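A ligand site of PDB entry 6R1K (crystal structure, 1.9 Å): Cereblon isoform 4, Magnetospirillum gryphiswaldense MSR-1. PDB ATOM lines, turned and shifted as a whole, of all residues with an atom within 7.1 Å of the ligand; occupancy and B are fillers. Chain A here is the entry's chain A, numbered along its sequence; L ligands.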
ATOM      1  N   VAL A  49       8.814 -18.677 -27.408  1.00  0.00           N
ATOM      2  CA  VAL A  49       9.940 -18.103 -28.171  1.00  0.00           C
ATOM      3  C   VAL A  49      11.242 -18.689 -27.680  1.00  0.00           C
ATOM      4  O   VAL A  49      11.298 -19.199 -26.566  1.00  0.00           O
ATOM      5  CB  VAL A  49       9.979 -16.549 -28.005  1.00  0.00           C
ATOM      6  CG1 VAL A  49       8.799 -15.911 -28.647  1.00  0.00           C
ATOM      7  CG2 VAL A  49       9.977 -16.135 -26.536  1.00  0.00           C
ATOM      8  N   PHE A  50      12.272 -18.636 -28.519  1.00  0.00           N
ATOM      9  CA  PHE A  50      13.606 -19.021 -28.148  1.00  0.00           C
ATOM     10  C   PHE A  50      14.621 -17.926 -28.408  1.00  0.00           C
ATOM     11  O   PHE A  50      14.495 -17.161 -29.364  1.00  0.00           O
ATOM     12  CB  PHE A  50      14.037 -20.327 -28.928  1.00  0.00           C
ATOM     13  N   ASN A  51      15.609 -17.834 -27.548  1.00  0.00           N
ATOM     14  CA  ASN A  51      16.705 -16.866 -27.682  1.00  0.00           C
ATOM     15  C   ASN A  51      17.891 -17.503 -28.420  1.00  0.00           C
ATOM     16  O   ASN A  51      17.831 -18.674 -28.806  1.00  0.00           O
ATOM     17  CB  ASN A  51      17.028 -16.237 -26.292  1.00  0.00           C
ATOM     18  CG  ASN A  51      17.783 -17.137 -25.366  1.00  0.00           C
ATOM     19  OD1 ASN A  51      18.145 -18.267 -25.686  1.00  0.00           O
ATOM     20  ND2 ASN A  51      18.099 -16.591 -24.200  1.00  0.00           N
ATOM     21  N   PRO A  52      18.966 -16.735 -28.640  1.00  0.00           N
ATOM     22  CA  PRO A  52      20.077 -17.308 -29.446  1.00  0.00           C
ATOM     23  C   PRO A  52      20.800 -18.460 -28.721  1.00  0.00           C
ATOM     24  O   PRO A  52      21.416 -19.276 -29.348  1.00  0.00           O
ATOM     25  CB  PRO A  52      20.997 -16.090 -29.651  1.00  0.00           C
ATOM     26  CG  PRO A  52      20.057 -14.897 -29.545  1.00  0.00           C
ATOM     27  CD  PRO A  52      19.124 -15.281 -28.440  1.00  0.00           C
ATOM     28  N   ALA A  53      20.672 -18.521 -27.397  1.00  0.00           N
ATOM     29  CA  ALA A  53      21.164 -19.637 -26.605  1.00  0.00           C
ATOM     30  C   ALA A  53      20.259 -20.878 -26.627  1.00  0.00           C
ATOM     31  O   ALA A  53      20.548 -21.871 -25.944  1.00  0.00           O
ATOM     32  CB  ALA A  53      21.400 -19.191 -25.164  1.00  0.00           C
ATOM     33  N   MET A  55      17.234 -21.155 -25.414  1.00  0.00           N
ATOM     34  CA  MET A  55      16.383 -21.231 -24.255  1.00  0.00           C
ATOM     35  C   MET A  55      14.971 -20.916 -24.718  1.00  0.00           C
ATOM     36  O   MET A  55      14.770 -19.879 -25.412  1.00  0.00           O
ATOM     37  CB  MET A  55      16.811 -20.218 -23.200  1.00  0.00           C
ATOM     38  CG  MET A  55      18.220 -20.389 -22.713  1.00  0.00           C
ATOM     39  SD  MET A  55      18.651 -18.971 -21.675  1.00  0.00           S
ATOM     40  CE  MET A  55      20.363 -19.411 -21.315  1.00  0.00           C
ATOM     41  N   PHE A  57      11.130 -19.891 -23.871  1.00  0.00           N
ATOM     42  CA  PHE A  57      10.406 -19.114 -22.889  1.00  0.00           C
ATOM     43  C   PHE A  57       8.991 -19.098 -23.334  1.00  0.00           C
ATOM     44  O   PHE A  57       8.689 -18.885 -24.521  1.00  0.00           O
ATOM     45  CB  PHE A  57      10.916 -17.679 -22.781  1.00  0.00           C
ATOM     46  CG  PHE A  57      12.368 -17.538 -22.444  1.00  0.00           C
ATOM     47  CD1 PHE A  57      12.786 -17.557 -21.118  1.00  0.00           C
ATOM     48  CD2 PHE A  57      13.315 -17.362 -23.436  1.00  0.00           C
ATOM     49  CE1 PHE A  57      14.103 -17.432 -20.792  1.00  0.00           C
ATOM     50  CE2 PHE A  57      14.674 -17.221 -23.101  1.00  0.00           C
ATOM     51  CZ  PHE A  57      15.048 -17.219 -21.761  1.00  0.00           C
ATOM     52  N   SER A  75      17.817  -2.877 -26.593  1.00  0.00           N
ATOM     53  CA  SER A  75      18.459  -3.495 -27.740  1.00  0.00           C
ATOM     54  C   SER A  75      17.371  -4.024 -28.636  1.00  0.00           C
ATOM     55  O   SER A  75      16.406  -4.648 -28.134  1.00  0.00           O
ATOM     56  CB  SER A  75      19.362  -4.674 -27.281  1.00  0.00           C
ATOM     57  OG  SER A  75      19.897  -5.326 -28.439  1.00  0.00           O
ATOM     58  N   GLY A  76      17.513  -3.832 -29.928  1.00  0.00           N
ATOM     59  CA  GLY A  76      16.635  -4.450 -30.926  1.00  0.00           C
ATOM     60  C   GLY A  76      17.085  -5.850 -31.295  1.00  0.00           C
ATOM     61  O   GLY A  76      16.333  -6.580 -31.915  1.00  0.00           O
ATOM     62  N   GLU A  77      18.308  -6.236 -30.939  1.00  0.00           N
ATOM     63  CA  GLU A  77      18.925  -7.482 -31.452  1.00  0.00           C
ATOM     64  C   GLU A  77      18.080  -8.694 -31.053  1.00  0.00           C
ATOM     65  O   GLU A  77      17.694  -8.852 -29.893  1.00  0.00           O
ATOM     66  CB  GLU A  77      20.332  -7.661 -30.907  1.00  0.00           C
ATOM     67  CG  GLU A  77      21.320  -6.696 -31.498  1.00  0.00           C
ATOM     68  CD  GLU A  77      22.644  -6.610 -30.724  1.00  0.00           C
ATOM     69  OE1 GLU A  77      23.033  -7.628 -30.095  1.00  0.00           O
ATOM     70  OE2 GLU A  77      23.307  -5.530 -30.751  1.00  0.00           O
ATOM     71  N   PHE A  78      17.709  -9.474 -32.049  1.00  0.00           N
ATOM     72  CA  PHE A  78      16.925 -10.703 -31.880  1.00  0.00           C
ATOM     73  C   PHE A  78      15.536 -10.459 -31.285  1.00  0.00           C
ATOM     74  O   PHE A  78      14.916 -11.396 -30.758  1.00  0.00           O
ATOM     75  CB  PHE A  78      17.659 -11.737 -30.979  1.00  0.00           C
ATOM     76  CG  PHE A  78      19.094 -11.942 -31.325  1.00  0.00           C
ATOM     77  CD1 PHE A  78      19.421 -12.583 -32.470  1.00  0.00           C
ATOM     78  CD2 PHE A  78      20.104 -11.504 -30.491  1.00  0.00           C
ATOM     79  CE1 PHE A  78      20.750 -12.786 -32.838  1.00  0.00           C
ATOM     80  CE2 PHE A  78      21.436 -11.677 -30.820  1.00  0.00           C
ATOM     81  CZ  PHE A  78      21.762 -12.311 -32.002  1.00  0.00           C
ATOM     82  N   SER A  79      15.018  -9.235 -31.332  1.00  0.00           N
ATOM     83  CA  SER A  79      13.760  -8.965 -30.714  1.00  0.00           C
ATOM     84  C   SER A  79      12.684  -9.873 -31.268  1.00  0.00           C
ATOM     85  O   SER A  79      12.576 -10.037 -32.469  1.00  0.00           O
ATOM     86  CB  SER A  79      13.310  -7.526 -30.865  1.00  0.00           C
ATOM     87  OG  SER A  79      12.077  -7.369 -30.218  1.00  0.00           O
ATOM     88  N   TRP A  80      11.862 -10.420 -30.385  1.00  0.00           N
ATOM     89  CA  TRP A  80      10.762 -11.282 -30.787  1.00  0.00           C
ATOM     90  C   TRP A  80       9.567 -10.493 -31.233  1.00  0.00           C
ATOM     91  O   TRP A  80       8.615 -11.079 -31.737  1.00  0.00           O
ATOM     92  CB  TRP A  80      10.336 -12.195 -29.646  1.00  0.00           C
ATOM     93  CG  TRP A  80      11.346 -13.166 -29.229  1.00  0.00           C
ATOM     94  CD1 TRP A  80      12.026 -14.025 -30.004  1.00  0.00           C
ATOM     95  CD2 TRP A  80      11.790 -13.360 -27.910  1.00  0.00           C
ATOM     96  NE1 TRP A  80      12.889 -14.785 -29.233  1.00  0.00           N
ATOM     97  CE2 TRP A  80      12.736 -14.398 -27.930  1.00  0.00           C
ATOM     98  CE3 TRP A  80      11.452 -12.777 -26.678  1.00  0.00           C
ATOM     99  CZ2 TRP A  80      13.348 -14.844 -26.775  1.00  0.00           C
ATOM    100  CZ3 TRP A  80      12.051 -13.223 -25.559  1.00  0.00           C
ATOM    101  CH2 TRP A  80      13.009 -14.231 -25.597  1.00  0.00           C
ATOM    102  N   PHE A  81       9.523  -9.175 -30.980  1.00  0.00           N
ATOM    103  CA  PHE A  81       8.329  -8.408 -31.281  1.00  0.00           C
ATOM    104  C   PHE A  81       8.767  -7.290 -32.213  1.00  0.00           C
ATOM    105  O   PHE A  81       9.595  -6.441 -31.878  1.00  0.00           O
ATOM    106  CB  PHE A  81       7.689  -7.896 -30.005  1.00  0.00           C
ATOM    107  CG  PHE A  81       7.260  -8.972 -29.065  1.00  0.00           C
ATOM    108  CD1 PHE A  81       8.118  -9.469 -28.113  1.00  0.00           C
ATOM    109  CD2 PHE A  81       5.961  -9.492 -29.126  1.00  0.00           C
ATOM    110  CE1 PHE A  81       7.718 -10.471 -27.227  1.00  0.00           C
ATOM    111  CE2 PHE A  81       5.559 -10.509 -28.260  1.00  0.00           C
ATOM    112  CZ  PHE A  81       6.419 -10.979 -27.297  1.00  0.00           C
ATOM    113  N   TYR A  84      10.052  -3.406 -31.625  1.00  0.00           N
ATOM    114  CA  TYR A  84      10.362  -3.155 -30.227  1.00  0.00           C
ATOM    115  C   TYR A  84      11.764  -3.521 -29.878  1.00  0.00           C
ATOM    116  O   TYR A  84      12.280  -4.543 -30.357  1.00  0.00           O
ATOM    117  CB  TYR A  84       9.439  -3.894 -29.306  1.00  0.00           C
ATOM    118  CG  TYR A  84       7.999  -3.530 -29.402  1.00  0.00           C
ATOM    119  CD1 TYR A  84       7.182  -4.205 -30.289  1.00  0.00           C
ATOM    120  CD2 TYR A  84       7.438  -2.531 -28.595  1.00  0.00           C
ATOM    121  CE1 TYR A  84       5.823  -3.911 -30.417  1.00  0.00           C
ATOM    122  CE2 TYR A  84       6.121  -2.187 -28.739  1.00  0.00           C
ATOM    123  CZ  TYR A  84       5.317  -2.884 -29.689  1.00  0.00           C
ATOM    124  OH  TYR A  84       3.988  -2.615 -29.780  1.00  0.00           O
ATOM    125  N   ASP A  85      12.362  -2.692 -29.025  1.00  0.00           N
ATOM    126  CA  ASP A  85      13.635  -2.950 -28.410  1.00  0.00           C
ATOM    127  C   ASP A  85      13.364  -3.439 -26.971  1.00  0.00           C
ATOM    128  O   ASP A  85      12.358  -3.069 -26.382  1.00  0.00           O
ATOM    129  CB  ASP A  85      14.465  -1.682 -28.330  1.00  0.00           C
ATOM    130  CG  ASP A  85      14.716  -1.081 -29.704  1.00  0.00           C
ATOM    131  OD1 ASP A  85      15.149  -1.820 -30.558  1.00  0.00           O
ATOM    132  OD2 ASP A  85      14.332   0.131 -29.929  1.00  0.00           O
ATOM    133  N   TRP A  86      14.223  -4.309 -26.470  1.00  0.00           N
ATOM    134  CA  TRP A  86      13.990  -4.916 -25.161  1.00  0.00           C
ATOM    135  C   TRP A  86      15.053  -4.503 -24.184  1.00  0.00           C
ATOM    136  O   TRP A  86      16.220  -4.249 -24.551  1.00  0.00           O
ATOM    137  CB  TRP A  86      13.871  -6.464 -25.216  1.00  0.00           C
ATOM    138  CG  TRP A  86      14.991  -7.134 -25.974  1.00  0.00           C
ATOM    139  CD1 TRP A  86      14.994  -7.497 -27.270  1.00  0.00           C
ATOM    140  CD2 TRP A  86      16.252  -7.527 -25.440  1.00  0.00           C
ATOM    141  NE1 TRP A  86      16.225  -8.035 -27.623  1.00  0.00           N
ATOM    142  CE2 TRP A  86      17.013  -8.062 -26.514  1.00  0.00           C
ATOM    143  CE3 TRP A  86      16.842  -7.418 -24.178  1.00  0.00           C
ATOM    144  CZ2 TRP A  86      18.336  -8.509 -26.364  1.00  0.00           C
ATOM    145  CZ3 TRP A  86      18.168  -7.899 -24.038  1.00  0.00           C
ATOM    146  CH2 TRP A  86      18.887  -8.439 -25.130  1.00  0.00           C
ATOM    147  N   THR A  87      14.640  -4.515 -22.927  1.00  0.00           N
ATOM    148  CA  THR A  87      15.561  -4.454 -21.794  1.00  0.00           C
ATOM    149  C   THR A  87      15.206  -5.615 -20.884  1.00  0.00           C
ATOM    150  O   THR A  87      14.046  -5.985 -20.795  1.00  0.00           O
ATOM    151  CB  THR A  87      15.437  -3.143 -21.028  1.00  0.00           C
ATOM    152  OG1 THR A  87      14.105  -3.027 -20.542  1.00  0.00           O
ATOM    153  CG2 THR A  87      15.734  -1.970 -21.937  1.00  0.00           C
ATOM    154  N   ILE A  88      16.197  -6.199 -20.265  1.00  0.00           N
ATOM    155  CA  ILE A  88      15.994  -7.312 -19.370  1.00  0.00           C
ATOM    156  C   ILE A  88      15.296  -6.813 -18.089  1.00  0.00           C
ATOM    157  O   ILE A  88      15.706  -5.807 -17.518  1.00  0.00           O
ATOM    158  CB  ILE A  88      17.324  -7.964 -19.022  1.00  0.00           C
ATOM    159  CG1 ILE A  88      17.922  -8.655 -20.265  1.00  0.00           C
ATOM    160  CG2 ILE A  88      17.157  -8.986 -17.906  1.00  0.00           C
ATOM    161  CD1 ILE A  88      19.436  -8.740 -20.246  1.00  0.00           C
ATOM    162  N   HIS A  97      15.525 -13.497 -13.195  1.00  0.00           N
ATOM    163  CA  HIS A  97      15.131 -13.008 -14.512  1.00  0.00           C
ATOM    164  C   HIS A  97      13.656 -13.326 -14.788  1.00  0.00           C
ATOM    165  O   HIS A  97      13.290 -14.472 -14.972  1.00  0.00           O
ATOM    166  CB  HIS A  97      16.051 -13.640 -15.547  1.00  0.00           C
ATOM    167  CG  HIS A  97      15.713 -13.217 -16.938  1.00  0.00           C
ATOM    168  ND1 HIS A  97      15.843 -14.063 -18.015  1.00  0.00           N
ATOM    169  CD2 HIS A  97      15.161 -12.063 -17.403  1.00  0.00           C
ATOM    170  CE1 HIS A  97      15.449 -13.410 -19.097  1.00  0.00           C
ATOM    171  NE2 HIS A  97      15.004 -12.223 -18.751  1.00  0.00           N
ATOM    172  N   GLY A  99      11.701 -11.555 -17.214  1.00  0.00           N
ATOM    173  CA  GLY A  99      11.342 -11.312 -18.608  1.00  0.00           C
ATOM    174  C   GLY A  99      12.005 -10.076 -19.163  1.00  0.00           C
ATOM    175  O   GLY A  99      13.200  -9.858 -18.927  1.00  0.00           O
ATOM    176  N   TRP A 100      11.234  -9.329 -19.939  1.00  0.00           N
ATOM    177  CA  TRP A 100      11.732  -8.178 -20.665  1.00  0.00           C
ATOM    178  C   TRP A 100      10.709  -7.058 -20.644  1.00  0.00           C
ATOM    179  O   TRP A 100       9.497  -7.313 -20.638  1.00  0.00           O
ATOM    180  CB  TRP A 100      12.054  -8.567 -22.143  1.00  0.00           C
ATOM    181  CG  TRP A 100      13.039  -9.670 -22.235  1.00  0.00           C
ATOM    182  CD1 TRP A 100      14.398  -9.558 -22.367  1.00  0.00           C
ATOM    183  CD2 TRP A 100      12.755 -11.053 -22.193  1.00  0.00           C
ATOM    184  NE1 TRP A 100      14.969 -10.814 -22.384  1.00  0.00           N
ATOM    185  CE2 TRP A 100      13.976 -11.743 -22.290  1.00  0.00           C
ATOM    186  CE3 TRP A 100      11.571 -11.793 -22.076  1.00  0.00           C
ATOM    187  CZ2 TRP A 100      14.034 -13.121 -22.250  1.00  0.00           C
ATOM    188  CZ3 TRP A 100      11.672 -13.176 -21.995  1.00  0.00           C
ATOM    189  CH2 TRP A 100      12.868 -13.807 -22.063  1.00  0.00           C
ATOM    190  N   TYR A 102       9.569  -4.046 -23.199  1.00  0.00           N
ATOM    191  CA  TYR A 102       9.651  -3.751 -24.636  1.00  0.00           C
ATOM    192  C   TYR A 102       9.277  -2.279 -24.825  1.00  0.00           C
ATOM    193  O   TYR A 102       8.340  -1.837 -24.200  1.00  0.00           O
ATOM    194  CB  TYR A 102       8.734  -4.651 -25.445  1.00  0.00           C
ATOM    195  CG  TYR A 102       9.310  -6.042 -25.544  1.00  0.00           C
ATOM    196  CD1 TYR A 102      10.269  -6.356 -26.502  1.00  0.00           C
ATOM    197  CD2 TYR A 102       8.968  -6.991 -24.612  1.00  0.00           C
ATOM    198  CE1 TYR A 102      10.830  -7.622 -26.566  1.00  0.00           C
ATOM    199  CE2 TYR A 102       9.490  -8.247 -24.675  1.00  0.00           C
ATOM    200  CZ  TYR A 102      10.423  -8.567 -25.652  1.00  0.00           C
ATOM    201  OH  TYR A 102      10.971  -9.836 -25.651  1.00  0.00           O
HETATM  202  C1  LIG L   1      15.505 -12.077 -25.741  1.00  0.00           C
HETATM  203  C2  LIG L   1      17.582 -12.586 -24.632  1.00  0.00           C
HETATM  204  C3  LIG L   1      18.954 -12.112 -24.269  1.00  0.00           C
HETATM  205  C4  LIG L   1      19.286 -11.923 -22.929  1.00  0.00           C
HETATM  206  C5  LIG L   1      19.954 -11.959 -25.233  1.00  0.00           C
HETATM  207  C6  LIG L   1      21.240 -11.565 -24.883  1.00  0.00           C
HETATM  208  C7  LIG L   1      21.520 -11.363 -23.549  1.00  0.00           C
HETATM  209  C8  LIG L   1      20.556 -11.527 -22.564  1.00  0.00           C
HETATM  210  N1  LIG L   1      14.683 -11.758 -27.887  1.00  0.00           N
HETATM  211  N2  LIG L   1      16.806 -11.736 -25.285  1.00  0.00           N
HETATM  212  C9  LIG L   1      14.550 -10.866 -25.729  1.00  0.00           C
HETATM  213  O1  LIG L   1      16.480 -13.183 -27.683  1.00  0.00           O
HETATM  214  C10 LIG L   1      15.632 -12.445 -27.195  1.00  0.00           C
HETATM  215  C11 LIG L   1      14.000 -10.831 -27.127  1.00  0.00           C
HETATM  216  O2  LIG L   1      13.066 -10.181 -27.544  1.00  0.00           O
HETATM  217  O3  LIG L   1      17.189 -13.706 -24.317  1.00  0.00           O
HETATM  218 CL1  LIG L   1      19.628 -12.200 -26.931  1.00  0.00          CL
HETATM  219 CL2  LIG L   1      23.129 -10.896 -23.100  1.00  0.00          CL
HETATM  220 CL3  LIG L   1      18.070 -12.107 -21.682  1.00  0.00          CL
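The backbone NH (N) of Trp 86 is in hydrogen-bond range of the backbone carbonyl oxygen (O) of Ser 75 (2.8 Å).
The indole nitrogen of Trp 80 is in hydrogen-bond range of the backbone carbonyl oxygen of Phe 50 (2.9 Å).
The backbone NH (N) of Met 55 lies within hydrogen-bond range of the side-chain amide oxygen (OD1) of Asn 51 (3.0 Å).
The side-chain amide oxygen (OD1) of Asn 51 sits at hydrogen-bond distance from the backbone NH (N) of Ala 53 (3.1 Å).
The backbone carbonyl oxygen (O) of Phe 81 lies within hydrogen-bond range of the side-chain hydroxyl (OG) of Ser 79 (3.1 Å).
NE1 of Trp 86 is in hydrogen-bond range of O of Glu 77, 2.8 Å away.
O of Gly 99 lies within hydrogen-bond range of NE2 of His 97, 3.0 Å away.
The side-chain hydroxyl (OG) of Ser 79 sits at hydrogen-bond distance from the backbone carbonyl oxygen (O) of Tyr 84.
An oxygen (O2) of the ligand lies within hydrogen-bond range of the side-chain hydroxyl (OH) of Tyr 102, 2.8 Å away.
The backbone carbonyl oxygen (O) of Phe 78 is in hydrogen-bond range of a nitrogen (N1) of the ligand, 2.9 Å away.
N of Trp 80 lies within hydrogen-bond range of O2 of the ligand (3.1 Å).
An oxygen (O3) of the ligand sits at hydrogen-bond distance from the side-chain amide nitrogen of Asn 51, 3.0 Å away.
Residues that only touch the ligand: Trp 86, Trp 100, Pro 52, Ser 79, Ile 88 and His 97.
Hydrophobic or aromatic side chains within 4 Å of the ligand: Pro 52, Phe 78, Trp 80, Trp 86, Ile 88, His 97, Trp 100 and Tyr 102.
The nearest printed residue that does not touch the ligand is Phe 57 (4.5 Å).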
